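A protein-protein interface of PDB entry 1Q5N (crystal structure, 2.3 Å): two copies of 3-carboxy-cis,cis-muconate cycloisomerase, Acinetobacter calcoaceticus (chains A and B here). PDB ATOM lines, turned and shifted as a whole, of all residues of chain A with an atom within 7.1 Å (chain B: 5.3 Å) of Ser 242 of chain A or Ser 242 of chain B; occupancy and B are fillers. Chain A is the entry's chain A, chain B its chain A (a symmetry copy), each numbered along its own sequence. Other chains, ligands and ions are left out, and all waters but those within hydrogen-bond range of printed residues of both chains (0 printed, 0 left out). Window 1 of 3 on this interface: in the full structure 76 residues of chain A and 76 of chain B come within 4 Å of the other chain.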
ATOM      1  N   ARG A 183       6.677  12.771  12.860  1.00  0.00           N
ATOM      2  CA  ARG A 183       6.577  11.345  12.579  1.00  0.00           C
ATOM      3  C   ARG A 183       5.706  10.636  13.608  1.00  0.00           C
ATOM      4  O   ARG A 183       4.867   9.816  13.248  1.00  0.00           O
ATOM      5  CB  ARG A 183       7.953  10.704  12.585  1.00  0.00           C
ATOM      6  CG  ARG A 183       8.754  11.020  11.360  1.00  0.00           C
ATOM      7  CD  ARG A 183      10.167  10.411  11.480  1.00  0.00           C
ATOM      8  NE  ARG A 183      10.967  10.881  10.359  1.00  0.00           N
ATOM      9  CZ  ARG A 183      12.029  11.677  10.487  1.00  0.00           C
ATOM     10  NH1 ARG A 183      12.433  12.084  11.697  1.00  0.00           N
ATOM     11  NH2 ARG A 183      12.667  12.085   9.391  1.00  0.00           N
ATOM     12  N   ILE A 187       1.813   8.632  12.741  1.00  0.00           N
ATOM     13  CA  ILE A 187       1.555   7.187  12.760  1.00  0.00           C
ATOM     14  C   ILE A 187       0.474   6.766  13.757  1.00  0.00           C
ATOM     15  O   ILE A 187      -0.047   5.649  13.697  1.00  0.00           O
ATOM     16  CB  ILE A 187       2.849   6.362  13.136  1.00  0.00           C
ATOM     17  CG1 ILE A 187       3.223   6.606  14.605  1.00  0.00           C
ATOM     18  CG2 ILE A 187       3.988   6.736  12.239  1.00  0.00           C
ATOM     19  CD1 ILE A 187       4.288   5.636  15.081  1.00  0.00           C
ATOM     20  N   ASP A 235       3.259  -4.840   9.982  1.00  0.00           N
ATOM     21  CA  ASP A 235       3.792  -3.530   9.653  1.00  0.00           C
ATOM     22  C   ASP A 235       3.533  -2.492  10.759  1.00  0.00           C
ATOM     23  O   ASP A 235       4.370  -1.644  10.992  1.00  0.00           O
ATOM     24  CB  ASP A 235       3.181  -3.061   8.330  1.00  0.00           C
ATOM     25  CG  ASP A 235       1.671  -3.071   8.383  1.00  0.00           C
ATOM     26  OD1 ASP A 235       1.059  -4.187   8.439  1.00  0.00           O
ATOM     27  OD2 ASP A 235       1.113  -1.960   8.416  1.00  0.00           O
ATOM     28  N   ILE A 237       3.693  -2.796  14.036  1.00  0.00           N
ATOM     29  CA  ILE A 237       4.674  -2.977  15.090  1.00  0.00           C
ATOM     30  C   ILE A 237       6.041  -2.425  14.614  1.00  0.00           C
ATOM     31  O   ILE A 237       6.727  -1.661  15.340  1.00  0.00           O
ATOM     32  CB  ILE A 237       4.846  -4.488  15.435  1.00  0.00           C
ATOM     33  CG1 ILE A 237       3.522  -5.071  15.981  1.00  0.00           C
ATOM     34  CG2 ILE A 237       5.974  -4.689  16.449  1.00  0.00           C
ATOM     35  CD1 ILE A 237       2.968  -4.363  17.198  1.00  0.00           C
ATOM     36  N   VAL A 238       6.419  -2.813  13.397  1.00  0.00           N
ATOM     37  CA  VAL A 238       7.681  -2.417  12.833  1.00  0.00           C
ATOM     38  C   VAL A 238       7.720  -0.920  12.693  1.00  0.00           C
ATOM     39  O   VAL A 238       8.745  -0.279  12.991  1.00  0.00           O
ATOM     40  CB  VAL A 238       7.880  -3.086  11.458  1.00  0.00           C
ATOM     41  CG1 VAL A 238       9.229  -2.689  10.844  1.00  0.00           C
ATOM     42  CG2 VAL A 238       7.821  -4.589  11.641  1.00  0.00           C
ATOM     43  N   GLU A 239       6.585  -0.350  12.275  1.00  0.00           N
ATOM     44  CA  GLU A 239       6.519   1.079  12.041  1.00  0.00           C
ATOM     45  C   GLU A 239       6.816   1.866  13.305  1.00  0.00           C
ATOM     46  O   GLU A 239       7.571   2.858  13.263  1.00  0.00           O
ATOM     47  CB  GLU A 239       5.168   1.455  11.437  1.00  0.00           C
ATOM     48  CG  GLU A 239       5.017   2.947  11.140  1.00  0.00           C
ATOM     49  CD  GLU A 239       3.819   3.281  10.264  1.00  0.00           C
ATOM     50  OE1 GLU A 239       2.773   2.614  10.333  1.00  0.00           O
ATOM     51  OE2 GLU A 239       3.923   4.229   9.500  1.00  0.00           O
ATOM     52  N   ILE A 240       6.256   1.409  14.429  1.00  0.00           N
ATOM     53  CA  ILE A 240       6.513   2.072  15.703  1.00  0.00           C
ATOM     54  C   ILE A 240       8.030   1.952  16.029  1.00  0.00           C
ATOM     55  O   ILE A 240       8.663   2.946  16.405  1.00  0.00           O
ATOM     56  CB  ILE A 240       5.678   1.431  16.832  1.00  0.00           C
ATOM     57  CG1 ILE A 240       4.197   1.787  16.650  1.00  0.00           C
ATOM     58  CG2 ILE A 240       6.110   1.970  18.229  1.00  0.00           C
ATOM     59  CD1 ILE A 240       3.288   0.908  17.560  1.00  0.00           C
ATOM     60  N   ALA A 241       8.605   0.754  15.874  1.00  0.00           N
ATOM     61  CA  ALA A 241      10.049   0.554  16.145  1.00  0.00           C
ATOM     62  C   ALA A 241      10.893   1.444  15.222  1.00  0.00           C
ATOM     63  O   ALA A 241      11.862   2.032  15.667  1.00  0.00           O
ATOM     64  CB  ALA A 241      10.490  -0.961  15.961  1.00  0.00           C
ATOM     65  N   SER A 242      10.508   1.550  13.952  1.00  0.00           N
ATOM     66  CA  SER A 242      11.296   2.349  13.010  1.00  0.00           C
ATOM     67  C   SER A 242      11.425   3.835  13.404  1.00  0.00           C
ATOM     68  O   SER A 242      12.454   4.461  13.183  1.00  0.00           O
ATOM     69  CB  SER A 242      10.732   2.238  11.566  1.00  0.00           C
ATOM     70  OG  SER A 242       9.499   2.914  11.447  1.00  0.00           O
ATOM     71  N   VAL A 243      10.380   4.389  13.997  1.00  0.00           N
ATOM     72  CA  VAL A 243      10.395   5.783  14.415  1.00  0.00           C
ATOM     73  C   VAL A 243      11.269   5.939  15.689  1.00  0.00           C
ATOM     74  O   VAL A 243      12.033   6.892  15.813  1.00  0.00           O
ATOM     75  CB  VAL A 243       8.927   6.243  14.606  1.00  0.00           C
ATOM     76  CG1 VAL A 243       8.856   7.610  15.324  1.00  0.00           C
ATOM     77  CG2 VAL A 243       8.279   6.368  13.220  1.00  0.00           C
ATOM     78  N   LEU A 244      11.181   4.976  16.611  1.00  0.00           N
ATOM     79  CA  LEU A 244      11.993   5.005  17.814  1.00  0.00           C
ATOM     80  C   LEU A 244      13.453   4.880  17.357  1.00  0.00           C
ATOM     81  O   LEU A 244      14.323   5.535  17.901  1.00  0.00           O
ATOM     82  CB  LEU A 244      11.617   3.854  18.758  1.00  0.00           C
ATOM     83  CG  LEU A 244      10.154   3.992  19.244  1.00  0.00           C
ATOM     84  CD1 LEU A 244       9.807   2.708  20.044  1.00  0.00           C
ATOM     85  CD2 LEU A 244       9.927   5.315  20.070  1.00  0.00           C
ATOM     86  N   GLY A 245      13.702   4.045  16.349  1.00  0.00           N
ATOM     87  CA  GLY A 245      15.041   3.881  15.834  1.00  0.00           C
ATOM     88  C   GLY A 245      15.623   5.202  15.307  1.00  0.00           C
ATOM     89  O   GLY A 245      16.798   5.485  15.545  1.00  0.00           O
ATOM     90  N   ILE A 246      14.824   6.013  14.610  1.00  0.00           N
ATOM     91  CA  ILE A 246      15.312   7.271  14.093  1.00  0.00           C
ATOM     92  C   ILE A 246      15.610   8.242  15.236  1.00  0.00           C
ATOM     93  O   ILE A 246      16.615   8.958  15.215  1.00  0.00           O
ATOM     94  CB  ILE A 246      14.297   7.904  13.134  1.00  0.00           C
ATOM     95  CG1 ILE A 246      14.264   7.111  11.817  1.00  0.00           C
ATOM     96  CG2 ILE A 246      14.643   9.371  12.881  1.00  0.00           C
ATOM     97  CD1 ILE A 246      13.039   7.481  10.981  1.00  0.00           C
ATOM     98  N   ILE A 247      14.764   8.236  16.263  1.00  0.00           N
ATOM     99  CA  ILE A 247      14.991   9.128  17.385  1.00  0.00           C
ATOM    100  C   ILE A 247      16.296   8.743  18.069  1.00  0.00           C
ATOM    101  O   ILE A 247      17.082   9.614  18.448  1.00  0.00           O
ATOM    102  CB  ILE A 247      13.808   9.065  18.423  1.00  0.00           C
ATOM    103  CG1 ILE A 247      12.555   9.676  17.774  1.00  0.00           C
ATOM    104  CG2 ILE A 247      14.227   9.733  19.767  1.00  0.00           C
ATOM    105  CD1 ILE A 247      11.230   9.309  18.495  1.00  0.00           C
ATOM    106  N   MET A 306      16.675  -3.453  15.293  1.00  0.00           N
ATOM    107  CA  MET A 306      15.879  -3.156  14.111  1.00  0.00           C
ATOM    108  C   MET A 306      15.954  -4.352  13.147  1.00  0.00           C
ATOM    109  O   MET A 306      14.938  -4.696  12.516  1.00  0.00           O
ATOM    110  CB  MET A 306      16.395  -1.916  13.353  1.00  0.00           C
ATOM    111  CG  MET A 306      15.988  -0.551  13.901  1.00  0.00           C
ATOM    112  SD  MET A 306      14.186  -0.357  14.036  1.00  0.00           S
ATOM    113  CE  MET A 306      14.172  -0.231  15.646  1.00  0.00           C
ATOM    114  N   ILE A 309      13.356  -6.890  14.424  1.00  0.00           N
ATOM    115  CA  ILE A 309      11.979  -6.521  14.313  1.00  0.00           C
ATOM    116  C   ILE A 309      11.579  -6.637  12.826  1.00  0.00           C
ATOM    117  O   ILE A 309      10.474  -7.120  12.529  1.00  0.00           O
ATOM    118  CB  ILE A 309      11.791  -5.116  15.009  1.00  0.00           C
ATOM    119  CG1 ILE A 309      10.545  -5.139  15.888  1.00  0.00           C
ATOM    120  CG2 ILE A 309      11.701  -4.040  14.055  1.00  0.00           C
ATOM    121  CD1 ILE A 309       9.398  -5.621  15.158  1.00  0.00           C
ATOM    122  N   TYR A 310      12.469  -6.250  11.897  1.00  0.00           N
ATOM    123  CA  TYR A 310      12.195  -6.419  10.471  1.00  0.00           C
ATOM    124  C   TYR A 310      12.146  -7.903  10.045  1.00  0.00           C
ATOM    125  O   TYR A 310      11.296  -8.254   9.230  1.00  0.00           O
ATOM    126  CB  TYR A 310      13.223  -5.677   9.625  1.00  0.00           C
ATOM    127  CG  TYR A 310      12.835  -4.221   9.388  1.00  0.00           C
ATOM    128  CD1 TYR A 310      11.924  -3.865   8.374  1.00  0.00           C
ATOM    129  CD2 TYR A 310      13.334  -3.199  10.230  1.00  0.00           C
ATOM    130  CE1 TYR A 310      11.519  -2.545   8.210  1.00  0.00           C
ATOM    131  CE2 TYR A 310      12.926  -1.874  10.071  1.00  0.00           C
ATOM    132  CZ  TYR A 310      12.034  -1.554   9.071  1.00  0.00           C
ATOM    133  OH  TYR A 310      11.676  -0.249   8.938  1.00  0.00           O
ATOM    134  N   LEU A 331      10.730  -5.397  20.760  1.00  0.00           N
ATOM    135  CA  LEU A 331       9.982  -4.146  20.870  1.00  0.00           C
ATOM    136  C   LEU A 331      10.166  -3.449  22.212  1.00  0.00           C
ATOM    137  O   LEU A 331      10.522  -2.271  22.249  1.00  0.00           O
ATOM    138  CB  LEU A 331       8.483  -4.338  20.561  1.00  0.00           C
ATOM    139  CG  LEU A 331       7.634  -3.031  20.507  1.00  0.00           C
ATOM    140  CD1 LEU A 331       8.086  -2.124  19.358  1.00  0.00           C
ATOM    141  CD2 LEU A 331       6.143  -3.336  20.314  1.00  0.00           C
ATOM    142  N   ILE A 334      13.620  -1.783  22.481  1.00  0.00           N
ATOM    143  CA  ILE A 334      13.775  -0.578  21.651  1.00  0.00           C
ATOM    144  C   ILE A 334      13.167   0.639  22.370  1.00  0.00           C
ATOM    145  O   ILE A 334      13.808   1.680  22.469  1.00  0.00           O
ATOM    146  CB  ILE A 334      13.124  -0.788  20.260  1.00  0.00           C
ATOM    147  CG1 ILE A 334      13.817  -1.972  19.610  1.00  0.00           C
ATOM    148  CG2 ILE A 334      13.194   0.506  19.396  1.00  0.00           C
ATOM    149  CD1 ILE A 334      13.455  -2.253  18.208  1.00  0.00           C
ATOM    150  N   ILE B 237      17.118  10.003   5.062  1.00  0.00           N
ATOM    151  CA  ILE B 237      17.620   8.855   4.331  1.00  0.00           C
ATOM    152  C   ILE B 237      17.083   7.558   4.987  1.00  0.00           C
ATOM    153  O   ILE B 237      16.569   6.640   4.298  1.00  0.00           O
ATOM    154  CB  ILE B 237      19.179   8.814   4.362  1.00  0.00           C
ATOM    155  CG1 ILE B 237      19.765  10.058   3.655  1.00  0.00           C
ATOM    156  CG2 ILE B 237      19.702   7.534   3.707  1.00  0.00           C
ATOM    157  CD1 ILE B 237      19.321  10.245   2.221  1.00  0.00           C
ATOM    158  N   VAL B 238      17.204   7.498   6.312  1.00  0.00           N
ATOM    159  CA  VAL B 238      16.790   6.343   7.061  1.00  0.00           C
ATOM    160  C   VAL B 238      15.309   6.138   6.888  1.00  0.00           C
ATOM    161  O   VAL B 238      14.841   4.998   6.710  1.00  0.00           O
ATOM    162  CB  VAL B 238      17.130   6.528   8.553  1.00  0.00           C
ATOM    163  CG1 VAL B 238      16.711   5.298   9.369  1.00  0.00           C
ATOM    164  CG2 VAL B 238      18.625   6.744   8.682  1.00  0.00           C
ATOM    165  N   GLU B 239      14.569   7.250   6.897  1.00  0.00           N
ATOM    166  CA  GLU B 239      13.124   7.176   6.803  1.00  0.00           C
ATOM    167  C   GLU B 239      12.682   6.518   5.508  1.00  0.00           C
ATOM    168  O   GLU B 239      11.772   5.665   5.516  1.00  0.00           O
ATOM    169  CB  GLU B 239      12.509   8.562   6.980  1.00  0.00           C
ATOM    170  CG  GLU B 239      10.982   8.575   6.912  1.00  0.00           C
ATOM    171  CD  GLU B 239      10.357   9.875   7.392  1.00  0.00           C
ATOM    172  OE1 GLU B 239      10.934  10.963   7.221  1.00  0.00           O
ATOM    173  OE2 GLU B 239       9.267   9.812   7.942  1.00  0.00           O
ATOM    174  N   ILE B 240      13.343   6.885   4.406  1.00  0.00           N
ATOM    175  CA  ILE B 240      13.021   6.280   3.117  1.00  0.00           C
ATOM    176  C   ILE B 240      13.336   4.757   3.190  1.00  0.00           C
ATOM    177  O   ILE B 240      12.513   3.934   2.773  1.00  0.00           O
ATOM    178  CB  ILE B 240      13.840   6.935   1.985  1.00  0.00           C
ATOM    179  CG1 ILE B 240      13.333   8.361   1.735  1.00  0.00           C
ATOM    180  CG2 ILE B 240      13.681   6.152   0.647  1.00  0.00           C
ATOM    181  CD1 ILE B 240      14.325   9.166   0.843  1.00  0.00           C
ATOM    182  N   ALA B 241      14.507   4.390   3.725  1.00  0.00           N
ATOM    183  CA  ALA B 241      14.880   2.961   3.848  1.00  0.00           C
ATOM    184  C   ALA B 241      13.869   2.221   4.735  1.00  0.00           C
ATOM    185  O   ALA B 241      13.481   1.111   4.417  1.00  0.00           O
ATOM    186  CB  ALA B 241      16.339   2.772   4.445  1.00  0.00           C
ATOM    187  N   SER B 242      13.437   2.847   5.828  1.00  0.00           N
ATOM    188  CA  SER B 242      12.505   2.177   6.738  1.00  0.00           C
ATOM    189  C   SER B 242      11.169   1.774   6.081  1.00  0.00           C
ATOM    190  O   SER B 242      10.593   0.741   6.401  1.00  0.00           O
ATOM    191  CB  SER B 242      12.229   3.042   7.999  1.00  0.00           C
ATOM    192  OG  SER B 242      11.446   4.173   7.680  1.00  0.00           O
ATOM    193  N   VAL B 243      10.688   2.589   5.157  1.00  0.00           N
ATOM    194  CA  VAL B 243       9.436   2.303   4.470  1.00  0.00           C
ATOM    195  C   VAL B 243       9.655   1.168   3.433  1.00  0.00           C
ATOM    196  O   VAL B 243       8.822   0.276   3.295  1.00  0.00           O
ATOM    197  CB  VAL B 243       8.917   3.624   3.847  1.00  0.00           C
ATOM    198  CG1 VAL B 243       7.756   3.362   2.861  1.00  0.00           C
ATOM    199  CG2 VAL B 243       8.418   4.527   4.983  1.00  0.00           C
ATOM    200  N   LEU B 244      10.797   1.185   2.741  1.00  0.00           N
ATOM    201  CA  LEU B 244      11.116   0.142   1.784  1.00  0.00           C
ATOM    202  C   LEU B 244      11.248  -1.160   2.587  1.00  0.00           C
ATOM    203  O   LEU B 244      10.811  -2.204   2.137  1.00  0.00           O
ATOM    204  CB  LEU B 244      12.423   0.459   1.041  1.00  0.00           C
ATOM    205  CG  LEU B 244      12.286   1.755   0.209  1.00  0.00           C
ATOM    206  CD1 LEU B 244      13.690   2.091  -0.362  1.00  0.00           C
ATOM    207  CD2 LEU B 244      11.180   1.627  -0.907  1.00  0.00           C
ATOM    208  N   GLY B 245      11.840  -1.079   3.777  1.00  0.00           N
ATOM    209  CA  GLY B 245      11.986  -2.246   4.616  1.00  0.00           C
ATOM    210  C   GLY B 245      10.629  -2.873   4.974  1.00  0.00           C
ATOM    211  O   GLY B 245      10.505  -4.099   4.965  1.00  0.00           O
ATOM    212  N   ILE B 246       9.616  -2.059   5.277  1.00  0.00           N
ATOM    213  CA  ILE B 246       8.314  -2.588   5.617  1.00  0.00           C
ATOM    214  C   ILE B 246       7.666  -3.246   4.398  1.00  0.00           C
ATOM    215  O   ILE B 246       7.049  -4.308   4.503  1.00  0.00           O
ATOM    216  CB  ILE B 246       7.395  -1.487   6.155  1.00  0.00           C
ATOM    217  CG1 ILE B 246       7.851  -1.073   7.564  1.00  0.00           C
ATOM    218  CG2 ILE B 246       5.942  -1.961   6.168  1.00  0.00           C
ATOM    219  CD1 ILE B 246       7.198   0.241   7.993  1.00  0.00           C
ATOM    220  N   MET B 306      19.095  -2.751   7.056  1.00  0.00           N
ATOM    221  CA  MET B 306      18.465  -1.770   7.928  1.00  0.00           C
ATOM    222  C   MET B 306      19.403  -1.483   9.112  1.00  0.00           C
ATOM    223  O   MET B 306      19.506  -0.320   9.545  1.00  0.00           O
ATOM    224  CB  MET B 306      17.127  -2.274   8.508  1.00  0.00           C
ATOM    225  CG  MET B 306      15.901  -2.174   7.605  1.00  0.00           C
ATOM    226  SD  MET B 306      15.600  -0.483   7.012  1.00  0.00           S
ATOM    227  CE  MET B 306      15.855  -0.825   5.455  1.00  0.00           C
ATOM    228  N   TYR B 310      20.668   2.406   9.880  1.00  0.00           N
ATOM    229  CA  TYR B 310      20.475   2.993  11.204  1.00  0.00           C
ATOM    230  C   TYR B 310      21.809   3.326  11.910  1.00  0.00           C
ATOM    231  O   TYR B 310      21.889   4.368  12.558  1.00  0.00           O
ATOM    232  CB  TYR B 310      19.641   2.078  12.092  1.00  0.00           C
ATOM    233  CG  TYR B 310      18.143   2.313  11.919  1.00  0.00           C
ATOM    234  CD1 TYR B 310      17.487   3.362  12.593  1.00  0.00           C
ATOM    235  CD2 TYR B 310      17.391   1.517  11.023  1.00  0.00           C
ATOM    236  CE1 TYR B 310      16.137   3.615  12.376  1.00  0.00           C
ATOM    237  CE2 TYR B 310      16.037   1.773  10.799  1.00  0.00           C
ATOM    238  CZ  TYR B 310      15.420   2.805  11.471  1.00  0.00           C
ATOM    239  OH  TYR B 310      14.096   3.008  11.238  1.00  0.00           O
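OH of Tyr 310 of chain A lies within hydrogen-bond range of O of Ser 242 of chain B.
The guanidinium group of Arg 183 of chain A lies within salt-bridge range of the side-chain carboxylate of Glu 239 of chain B.
O of Ser 242 of chain A is in hydrogen-bond range of OH of Tyr 310 of chain B.
The side-chain hydroxyl (OG) of Ser 242 of chain A sits at hydrogen-bond distance from the backbone carbonyl oxygen (O) of Glu 239 of chain A, 2.6 Å away.
The backbone carbonyl oxygen (O) of Glu 239 of chain B sits at hydrogen-bond distance from the side-chain hydroxyl (OG) of Ser 242 of chain B (2.6 Å).
Among the printed residues, pairs that only touch across the chains: Tyr 310 of chain A with Gly 245 of chain B (3.4 Å), Gly 245 of chain A with Tyr 310 of chain B (3.4 Å), Tyr 310 of chain A with Ile 246 of chain B (3.5 Å), Ile 246 of chain A with Tyr 310 of chain B (3.5 Å), Asp 235 of chain A with Ile 246 of chain B (3.7 Å), Met 306 of chain A with Tyr 310 of chain B (3.8 Å), Tyr 310 of chain A with Met 306 of chain B (3.8 Å), Ile 246 of chain A with Val 238 of chain B (3.9 Å), Val 238 of chain A with Ile 246 of chain B (3.9 Å) and Ser 242 of chain A with Ser 242 of chain B (3.95 Å).
Of chain B, only Ser 242 and Tyr 310 come within 4 Å of Ser 242 of chain A.
Ser 242 of chain B touches just these residues of chain A: Ser 242 (3.95 Å) and Tyr 310 (2.9 Å).
Of the printed residues of chain A, Val 238 of chain B touches Ile 246 (3.9 Å).
Printed residues of chain B within 4 Å of Arg 183 of chain A: Glu 239.
The nearest printed residue of chain B that does not touch Ile 246 of chain A is Glu 239 of chain B (4.2 Å).
Of the 19 printed residues of chain A, 8 touch a printed residue of chain B.
Hydrophobic or aromatic side chains of chain A within 4 Å of the printed part of chain B: Val 238, Ile 246, Met 306 and Tyr 310.
Of the 12 printed residues of chain B, 7 touch a printed residue of chain A.
Hydrophobic or aromatic side chains of chain B within 4 Å of the printed part of chain A: Val 238, Ile 246, Met 306 and Tyr 310.
Along chain B the printed residues that touch a printed residue of chain A span positions 238 to 310.
Among the printed residues, Asp or Glu carboxylates within 4 Å of a Lys or Arg side-chain nitrogen of the other chain: Arg 183 of chain A with Glu 239 of chain B (3.0 Å).
Ser 242 of chain A touches Tyr 310 of chain B, and with the chains exchanged Tyr 310 of chain A touches Ser 242 of chain B.
Gly 245 of chain A touches Tyr 310 of chain B, and with the chains exchanged Tyr 310 of chain A touches Gly 245 of chain B.
Ile 246 of chain A touches Tyr 310 of chain B, and with the chains exchanged Tyr 310 of chain A touches Ile 246 of chain B.
Met 306 of chain A touches Tyr 310 of chain B, and with the chains exchanged Tyr 310 of chain A touches Met 306 of chain B.
12 positions are printed for both chains.
Of the 13 pairs that touch across the chains among the printed residues, 11 have their exchanged pair printed and touching as well.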
